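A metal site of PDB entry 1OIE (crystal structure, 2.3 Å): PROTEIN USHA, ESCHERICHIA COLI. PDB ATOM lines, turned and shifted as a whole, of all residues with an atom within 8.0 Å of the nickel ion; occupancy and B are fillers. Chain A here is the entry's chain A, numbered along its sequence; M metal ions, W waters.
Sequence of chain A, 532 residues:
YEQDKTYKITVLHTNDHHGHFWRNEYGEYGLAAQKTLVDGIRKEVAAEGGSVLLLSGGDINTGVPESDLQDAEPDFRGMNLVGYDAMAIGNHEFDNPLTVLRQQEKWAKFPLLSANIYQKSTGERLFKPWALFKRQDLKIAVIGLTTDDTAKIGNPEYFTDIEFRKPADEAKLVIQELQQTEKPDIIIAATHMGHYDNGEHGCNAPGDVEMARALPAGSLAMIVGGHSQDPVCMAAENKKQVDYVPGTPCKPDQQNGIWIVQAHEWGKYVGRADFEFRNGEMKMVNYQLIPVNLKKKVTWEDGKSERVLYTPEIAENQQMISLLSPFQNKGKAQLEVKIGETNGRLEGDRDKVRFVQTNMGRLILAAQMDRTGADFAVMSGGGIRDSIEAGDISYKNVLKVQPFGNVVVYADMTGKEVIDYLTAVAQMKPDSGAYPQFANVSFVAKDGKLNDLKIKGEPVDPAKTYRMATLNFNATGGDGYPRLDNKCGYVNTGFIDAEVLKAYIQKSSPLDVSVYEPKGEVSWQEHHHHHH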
ATOM      1  N   ASP A  16      29.088  -5.039  -8.627  1.00  0.00           N
ATOM      2  CA  ASP A  16      27.717  -4.879  -8.248  1.00  0.00           C
ATOM      3  C   ASP A  16      26.917  -6.011  -8.853  1.00  0.00           C
ATOM      4  O   ASP A  16      25.856  -5.816  -9.473  1.00  0.00           O
ATOM      5  CB  ASP A  16      27.225  -3.514  -8.686  1.00  0.00           C
ATOM      6  CG  ASP A  16      27.983  -2.428  -8.002  1.00  0.00           C
ATOM      7  OD1 ASP A  16      27.490  -1.935  -6.957  1.00  0.00           O
ATOM      8  OD2 ASP A  16      29.107  -2.048  -8.403  1.00  0.00           O
ATOM      9  N   HIS A  18      25.329  -8.383  -7.203  1.00  0.00           N
ATOM     10  CA  HIS A  18      24.042  -8.350  -6.503  1.00  0.00           C
ATOM     11  C   HIS A  18      23.159  -9.580  -6.720  1.00  0.00           C
ATOM     12  O   HIS A  18      21.959  -9.452  -6.979  1.00  0.00           O
ATOM     13  CB  HIS A  18      23.251  -7.106  -6.909  1.00  0.00           C
ATOM     14  CG  HIS A  18      23.743  -5.868  -6.259  1.00  0.00           C
ATOM     15  ND1 HIS A  18      23.739  -5.699  -4.896  1.00  0.00           N
ATOM     16  CD2 HIS A  18      24.262  -4.727  -6.778  1.00  0.00           C
ATOM     17  CE1 HIS A  18      24.206  -4.496  -4.609  1.00  0.00           C
ATOM     18  NE2 HIS A  18      24.550  -3.896  -5.726  1.00  0.00           N
ATOM     19  N   GLY A  57      34.529  -5.162  -8.308  1.00  0.00           N
ATOM     20  CA  GLY A  57      34.295  -4.003  -7.512  1.00  0.00           C
ATOM     21  C   GLY A  57      33.333  -4.197  -6.364  1.00  0.00           C
ATOM     22  O   GLY A  57      32.918  -3.219  -5.784  1.00  0.00           O
ATOM     23  N   GLY A  58      32.933  -5.427  -6.083  1.00  0.00           N
ATOM     24  CA  GLY A  58      32.118  -5.689  -4.933  1.00  0.00           C
ATOM     25  C   GLY A  58      30.617  -5.552  -5.073  1.00  0.00           C
ATOM     26  O   GLY A  58      30.082  -5.318  -6.146  1.00  0.00           O
ATOM     27  N   ASP A  59      29.928  -5.626  -3.925  1.00  0.00           N
ATOM     28  CA  ASP A  59      28.475  -5.748  -3.881  1.00  0.00           C
ATOM     29  C   ASP A  59      28.072  -7.007  -4.585  1.00  0.00           C
ATOM     30  O   ASP A  59      27.398  -7.008  -5.568  1.00  0.00           O
ATOM     31  CB  ASP A  59      27.770  -4.520  -4.431  1.00  0.00           C
ATOM     32  CG  ASP A  59      27.499  -3.474  -3.370  1.00  0.00           C
ATOM     33  OD1 ASP A  59      27.956  -3.570  -2.196  1.00  0.00           O
ATOM     34  OD2 ASP A  59      26.854  -2.462  -3.633  1.00  0.00           O
ATOM     35  N   ASN A  61      26.622  -9.358  -2.627  1.00  0.00           N
ATOM     36  CA  ASN A  61      25.378  -9.562  -1.892  1.00  0.00           C
ATOM     37  C   ASN A  61      24.230  -8.668  -2.318  1.00  0.00           C
ATOM     38  O   ASN A  61      24.421  -7.491  -2.675  1.00  0.00           O
ATOM     39  CB  ASN A  61      25.622  -9.280  -0.409  1.00  0.00           C
ATOM     40  CG  ASN A  61      26.404 -10.377   0.276  1.00  0.00           C
ATOM     41  OD1 ASN A  61      25.825 -11.364   0.736  1.00  0.00           O
ATOM     42  ND2 ASN A  61      27.723 -10.189   0.400  1.00  0.00           N
ATOM     43  N   ILE A  89      35.437  -5.003  -1.079  1.00  0.00           N
ATOM     44  CA  ILE A  89      34.262  -5.136  -0.262  1.00  0.00           C
ATOM     45  C   ILE A  89      33.289  -3.952  -0.516  1.00  0.00           C
ATOM     46  O   ILE A  89      33.678  -2.746  -0.476  1.00  0.00           O
ATOM     47  CB  ILE A  89      34.694  -5.198   1.215  1.00  0.00           C
ATOM     48  CG1 ILE A  89      35.465  -6.520   1.497  1.00  0.00           C
ATOM     49  CG2 ILE A  89      33.500  -5.110   2.146  1.00  0.00           C
ATOM     50  CD1 ILE A  89      36.022  -6.580   2.881  1.00  0.00           C
ATOM     51  N   GLY A  90      32.054  -4.281  -0.801  1.00  0.00           N
ATOM     52  CA  GLY A  90      31.043  -3.261  -1.023  1.00  0.00           C
ATOM     53  C   GLY A  90      30.246  -2.976   0.229  1.00  0.00           C
ATOM     54  O   GLY A  90      30.340  -3.715   1.195  1.00  0.00           O
ATOM     55  N   ASN A  91      29.440  -1.917   0.204  1.00  0.00           N
ATOM     56  CA  ASN A  91      28.575  -1.628   1.297  1.00  0.00           C
ATOM     57  C   ASN A  91      27.546  -2.745   1.532  1.00  0.00           C
ATOM     58  O   ASN A  91      27.183  -3.005   2.659  1.00  0.00           O
ATOM     59  CB  ASN A  91      27.916  -0.240   1.157  1.00  0.00           C
ATOM     60  CG  ASN A  91      27.109  -0.107  -0.125  1.00  0.00           C
ATOM     61  OD1 ASN A  91      27.550  -0.486  -1.142  1.00  0.00           O
ATOM     62  ND2 ASN A  91      25.917   0.426  -0.030  1.00  0.00           N
ATOM     63  N   HIS A  92      27.106  -3.415   0.473  1.00  0.00           N
ATOM     64  CA  HIS A  92      26.099  -4.451   0.641  1.00  0.00           C
ATOM     65  C   HIS A  92      26.655  -5.713   1.233  1.00  0.00           C
ATOM     66  O   HIS A  92      25.902  -6.530   1.658  1.00  0.00           O
ATOM     67  CB  HIS A  92      25.325  -4.688  -0.623  1.00  0.00           C
ATOM     68  CG  HIS A  92      24.335  -3.600  -0.922  1.00  0.00           C
ATOM     69  ND1 HIS A  92      23.077  -3.594  -0.385  1.00  0.00           N
ATOM     70  CD2 HIS A  92      24.452  -2.437  -1.619  1.00  0.00           C
ATOM     71  CE1 HIS A  92      22.431  -2.504  -0.764  1.00  0.00           C
ATOM     72  NE2 HIS A  92      23.242  -1.783  -1.527  1.00  0.00           N
ATOM     73  N   GLU A  93      27.983  -5.855   1.297  1.00  0.00           N
ATOM     74  CA  GLU A  93      28.584  -6.936   2.049  1.00  0.00           C
ATOM     75  C   GLU A  93      28.308  -6.774   3.549  1.00  0.00           C
ATOM     76  O   GLU A  93      28.618  -7.694   4.349  1.00  0.00           O
ATOM     77  CB  GLU A  93      30.113  -6.963   1.844  1.00  0.00           C
ATOM     78  CG  GLU A  93      30.635  -7.803   0.667  1.00  0.00           C
ATOM     79  CD  GLU A  93      30.037  -7.482  -0.670  1.00  0.00           C
ATOM     80  OE1 GLU A  93      29.093  -8.190  -1.045  1.00  0.00           O
ATOM     81  OE2 GLU A  93      30.577  -6.620  -1.396  1.00  0.00           O
ATOM     82  N   THR A 146      36.468   0.848   0.266  1.00  0.00           N
ATOM     83  CA  THR A 146      35.042   0.797   0.414  1.00  0.00           C
ATOM     84  C   THR A 146      34.525   2.195   0.761  1.00  0.00           C
ATOM     85  O   THR A 146      35.113   2.860   1.585  1.00  0.00           O
ATOM     86  CB  THR A 146      34.680  -0.177   1.519  1.00  0.00           C
ATOM     87  OG1 THR A 146      35.287  -1.470   1.256  1.00  0.00           O
ATOM     88  CG2 THR A 146      33.176  -0.378   1.590  1.00  0.00           C
ATOM     89  N   THR A 147      33.393   2.581   0.174  1.00  0.00           N
ATOM     90  CA  THR A 147      32.820   3.910   0.398  1.00  0.00           C
ATOM     91  C   THR A 147      32.516   4.105   1.851  1.00  0.00           C
ATOM     92  O   THR A 147      32.015   3.188   2.523  1.00  0.00           O
ATOM     93  CB  THR A 147      31.535   4.130  -0.424  1.00  0.00           C
ATOM     94  OG1 THR A 147      30.930   5.373  -0.044  1.00  0.00           O
ATOM     95  CG2 THR A 147      30.481   3.097  -0.154  1.00  0.00           C
ATOM     96  N   THR A 150      29.062   3.761   3.803  1.00  0.00           N
ATOM     97  CA  THR A 150      28.467   2.445   4.084  1.00  0.00           C
ATOM     98  C   THR A 150      27.577   2.450   5.312  1.00  0.00           C
ATOM     99  O   THR A 150      26.410   1.998   5.269  1.00  0.00           O
ATOM    100  CB  THR A 150      29.568   1.434   4.214  1.00  0.00           C
ATOM    101  OG1 THR A 150      30.182   1.242   2.923  1.00  0.00           O
ATOM    102  CG2 THR A 150      29.046   0.083   4.571  1.00  0.00           C
ATOM    103  N   ILE A 153      24.142   5.138   5.547  1.00  0.00           N
ATOM    104  CA  ILE A 153      23.041   5.006   4.598  1.00  0.00           C
ATOM    105  C   ILE A 153      21.883   4.205   5.185  1.00  0.00           C
ATOM    106  O   ILE A 153      22.087   3.213   5.833  1.00  0.00           O
ATOM    107  CB  ILE A 153      23.556   4.217   3.385  1.00  0.00           C
ATOM    108  CG1 ILE A 153      24.330   5.114   2.423  1.00  0.00           C
ATOM    109  CG2 ILE A 153      22.418   3.550   2.637  1.00  0.00           C
ATOM    110  CD1 ILE A 153      24.934   4.247   1.183  1.00  0.00           C
ATOM    111  N   HIS A 192      34.832   0.364  -4.265  1.00  0.00           N
ATOM    112  CA  HIS A 192      33.400   0.422  -4.171  1.00  0.00           C
ATOM    113  C   HIS A 192      32.951   1.818  -3.686  1.00  0.00           C
ATOM    114  O   HIS A 192      32.408   2.000  -2.628  1.00  0.00           O
ATOM    115  CB  HIS A 192      32.872  -0.704  -3.290  1.00  0.00           C
ATOM    116  CG  HIS A 192      31.424  -0.898  -3.491  1.00  0.00           C
ATOM    117  ND1 HIS A 192      30.939  -1.652  -4.543  1.00  0.00           N
ATOM    118  CD2 HIS A 192      30.354  -0.335  -2.876  1.00  0.00           C
ATOM    119  CE1 HIS A 192      29.618  -1.562  -4.561  1.00  0.00           C
ATOM    120  NE2 HIS A 192      29.245  -0.758  -3.571  1.00  0.00           N
ATOM    121  N   MET A 193      33.236   2.807  -4.528  1.00  0.00           N
ATOM    122  CA  MET A 193      33.115   4.195  -4.203  1.00  0.00           C
ATOM    123  C   MET A 193      32.239   5.035  -5.161  1.00  0.00           C
ATOM    124  O   MET A 193      31.671   6.033  -4.736  1.00  0.00           O
ATOM    125  CB  MET A 193      34.499   4.797  -4.157  1.00  0.00           C
ATOM    126  CG  MET A 193      35.405   4.155  -3.088  1.00  0.00           C
ATOM    127  SD  MET A 193      37.028   4.911  -3.010  1.00  0.00           S
ATOM    128  CE  MET A 193      37.609   4.489  -4.223  1.00  0.00           C
ATOM    129  N   GLY A 194      32.183   4.663  -6.434  1.00  0.00           N
ATOM    130  CA  GLY A 194      31.339   5.367  -7.401  1.00  0.00           C
ATOM    131  C   GLY A 194      32.058   6.308  -8.359  1.00  0.00           C
ATOM    132  O   GLY A 194      32.980   7.028  -8.032  1.00  0.00           O
ATOM    133  N   GLY A 226      32.810   0.480  -8.811  1.00  0.00           N
ATOM    134  CA  GLY A 226      31.465  -0.024  -8.592  1.00  0.00           C
ATOM    135  C   GLY A 226      30.625   0.976  -7.798  1.00  0.00           C
ATOM    136  O   GLY A 226      30.948   2.147  -7.759  1.00  0.00           O
ATOM    137  N   HIS A 227      29.532   0.469  -7.185  1.00  0.00           N
ATOM    138  CA  HIS A 227      28.688   1.192  -6.267  1.00  0.00           C
ATOM    139  C   HIS A 227      27.685   2.058  -7.010  1.00  0.00           C
ATOM    140  O   HIS A 227      26.476   1.891  -6.805  1.00  0.00           O
ATOM    141  CB  HIS A 227      29.504   2.005  -5.291  1.00  0.00           C
ATOM    142  CG  HIS A 227      28.684   2.699  -4.255  1.00  0.00           C
ATOM    143  ND1 HIS A 227      27.718   2.056  -3.534  1.00  0.00           N
ATOM    144  CD2 HIS A 227      28.640   4.003  -3.867  1.00  0.00           C
ATOM    145  CE1 HIS A 227      27.130   2.919  -2.715  1.00  0.00           C
ATOM    146  NE2 HIS A 227      27.682   4.102  -2.872  1.00  0.00           N
ATOM    147  N   SER A 228      28.207   2.957  -7.874  1.00  0.00           N
ATOM    148  CA  SER A 228      27.361   3.877  -8.638  1.00  0.00           C
ATOM    149  C   SER A 228      26.593   3.102  -9.684  1.00  0.00           C
ATOM    150  O   SER A 228      25.518   3.538 -10.059  1.00  0.00           O
ATOM    151  CB  SER A 228      28.159   5.031  -9.285  1.00  0.00           C
ATOM    152  OG  SER A 228      29.180   4.542 -10.174  1.00  0.00           O
ATOM    153  N   GLN A 229      27.128   1.965 -10.136  1.00  0.00           N
ATOM    154  CA  GLN A 229      26.445   1.038 -11.053  1.00  0.00           C
ATOM    155  C   GLN A 229      26.196   1.707 -12.440  1.00  0.00           C
ATOM    156  O   GLN A 229      25.066   1.984 -12.852  1.00  0.00           O
ATOM    157  CB  GLN A 229      25.119   0.488 -10.406  1.00  0.00           C
ATOM    158  CG  GLN A 229      25.381  -0.494  -9.248  1.00  0.00           C
ATOM    159  CD  GLN A 229      24.144  -0.997  -8.491  1.00  0.00           C
ATOM    160  OE1 GLN A 229      24.126  -0.954  -7.255  1.00  0.00           O
ATOM    161  NE2 GLN A 229      23.152  -1.542  -9.216  1.00  0.00           N
ATOM    162  N   ASN A 492      19.633   5.925  -3.699  1.00  0.00           N
ATOM    163  CA  ASN A 492      19.151   4.627  -4.172  1.00  0.00           C
ATOM    164  C   ASN A 492      19.842   3.576  -3.261  1.00  0.00           C
ATOM    165  O   ASN A 492      21.022   3.506  -3.259  1.00  0.00           O
ATOM    166  CB  ASN A 492      19.520   4.452  -5.636  1.00  0.00           C
ATOM    167  CG  ASN A 492      19.131   3.072  -6.207  1.00  0.00           C
ATOM    168  OD1 ASN A 492      19.305   2.025  -5.571  1.00  0.00           O
ATOM    169  ND2 ASN A 492      18.559   3.070  -7.353  1.00  0.00           N
ATOM    170  N   THR A 493      19.108   2.788  -2.485  1.00  0.00           N
ATOM    171  CA  THR A 493      19.720   1.878  -1.513  1.00  0.00           C
ATOM    172  C   THR A 493      20.119   0.582  -2.111  1.00  0.00           C
ATOM    173  O   THR A 493      20.840  -0.141  -1.493  1.00  0.00           O
ATOM    174  CB  THR A 493      18.739   1.502  -0.395  1.00  0.00           C
ATOM    175  OG1 THR A 493      17.620   0.749  -0.898  1.00  0.00           O
ATOM    176  CG2 THR A 493      18.118   2.696   0.224  1.00  0.00           C
ATOM    177  N   GLY A 494      19.551   0.226  -3.268  1.00  0.00           N
ATOM    178  CA  GLY A 494      19.823  -1.035  -3.901  1.00  0.00           C
ATOM    179  C   GLY A 494      18.973  -2.161  -3.342  1.00  0.00           C
ATOM    180  O   GLY A 494      19.141  -3.334  -3.746  1.00  0.00           O
HETATM  181 NI    NI M   1      27.379  -0.200  -3.325  1.00  0.00          NI
HETATM  182  O   HOH W   1      25.395  -0.031  -4.502  1.00  0.00           O
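The backbone NH (N) of Thr 147 is in hydrogen-bond range of the backbone carbonyl oxygen (O) of His 192 (3.0 Å). ND1 of His 192 lies within hydrogen-bond range of O of Gly 57. OD2 of Asp 16 sits at hydrogen-bond distance from N of His 227, at 2.8 Å. The side-chain carboxylate (OD1) of Asp 59 sits at hydrogen-bond distance from the backbone NH (N) of His 92 (2.8 Å). The backbone NH (N) of His 18 sits at hydrogen-bond distance from the backbone carbonyl oxygen (O) of Asp 59. N of Asp 59 is in hydrogen-bond range of OE2 of Glu 93.
The nickel ion is bound by NE2 of His 192 (2.0 Å), OD1 of Asn 91 (2.2 Å), ND1 of His 227 (2.3 Å), water W1 (2.3 Å) and OD2 of Asp 59 (2.3 Å). The nickel ion has five donor atoms within binding distance.
Water W1 lies within hydrogen-bond range of OE1 of Gln 229 (3.2 Å) and O of His 227 (3.2 Å).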
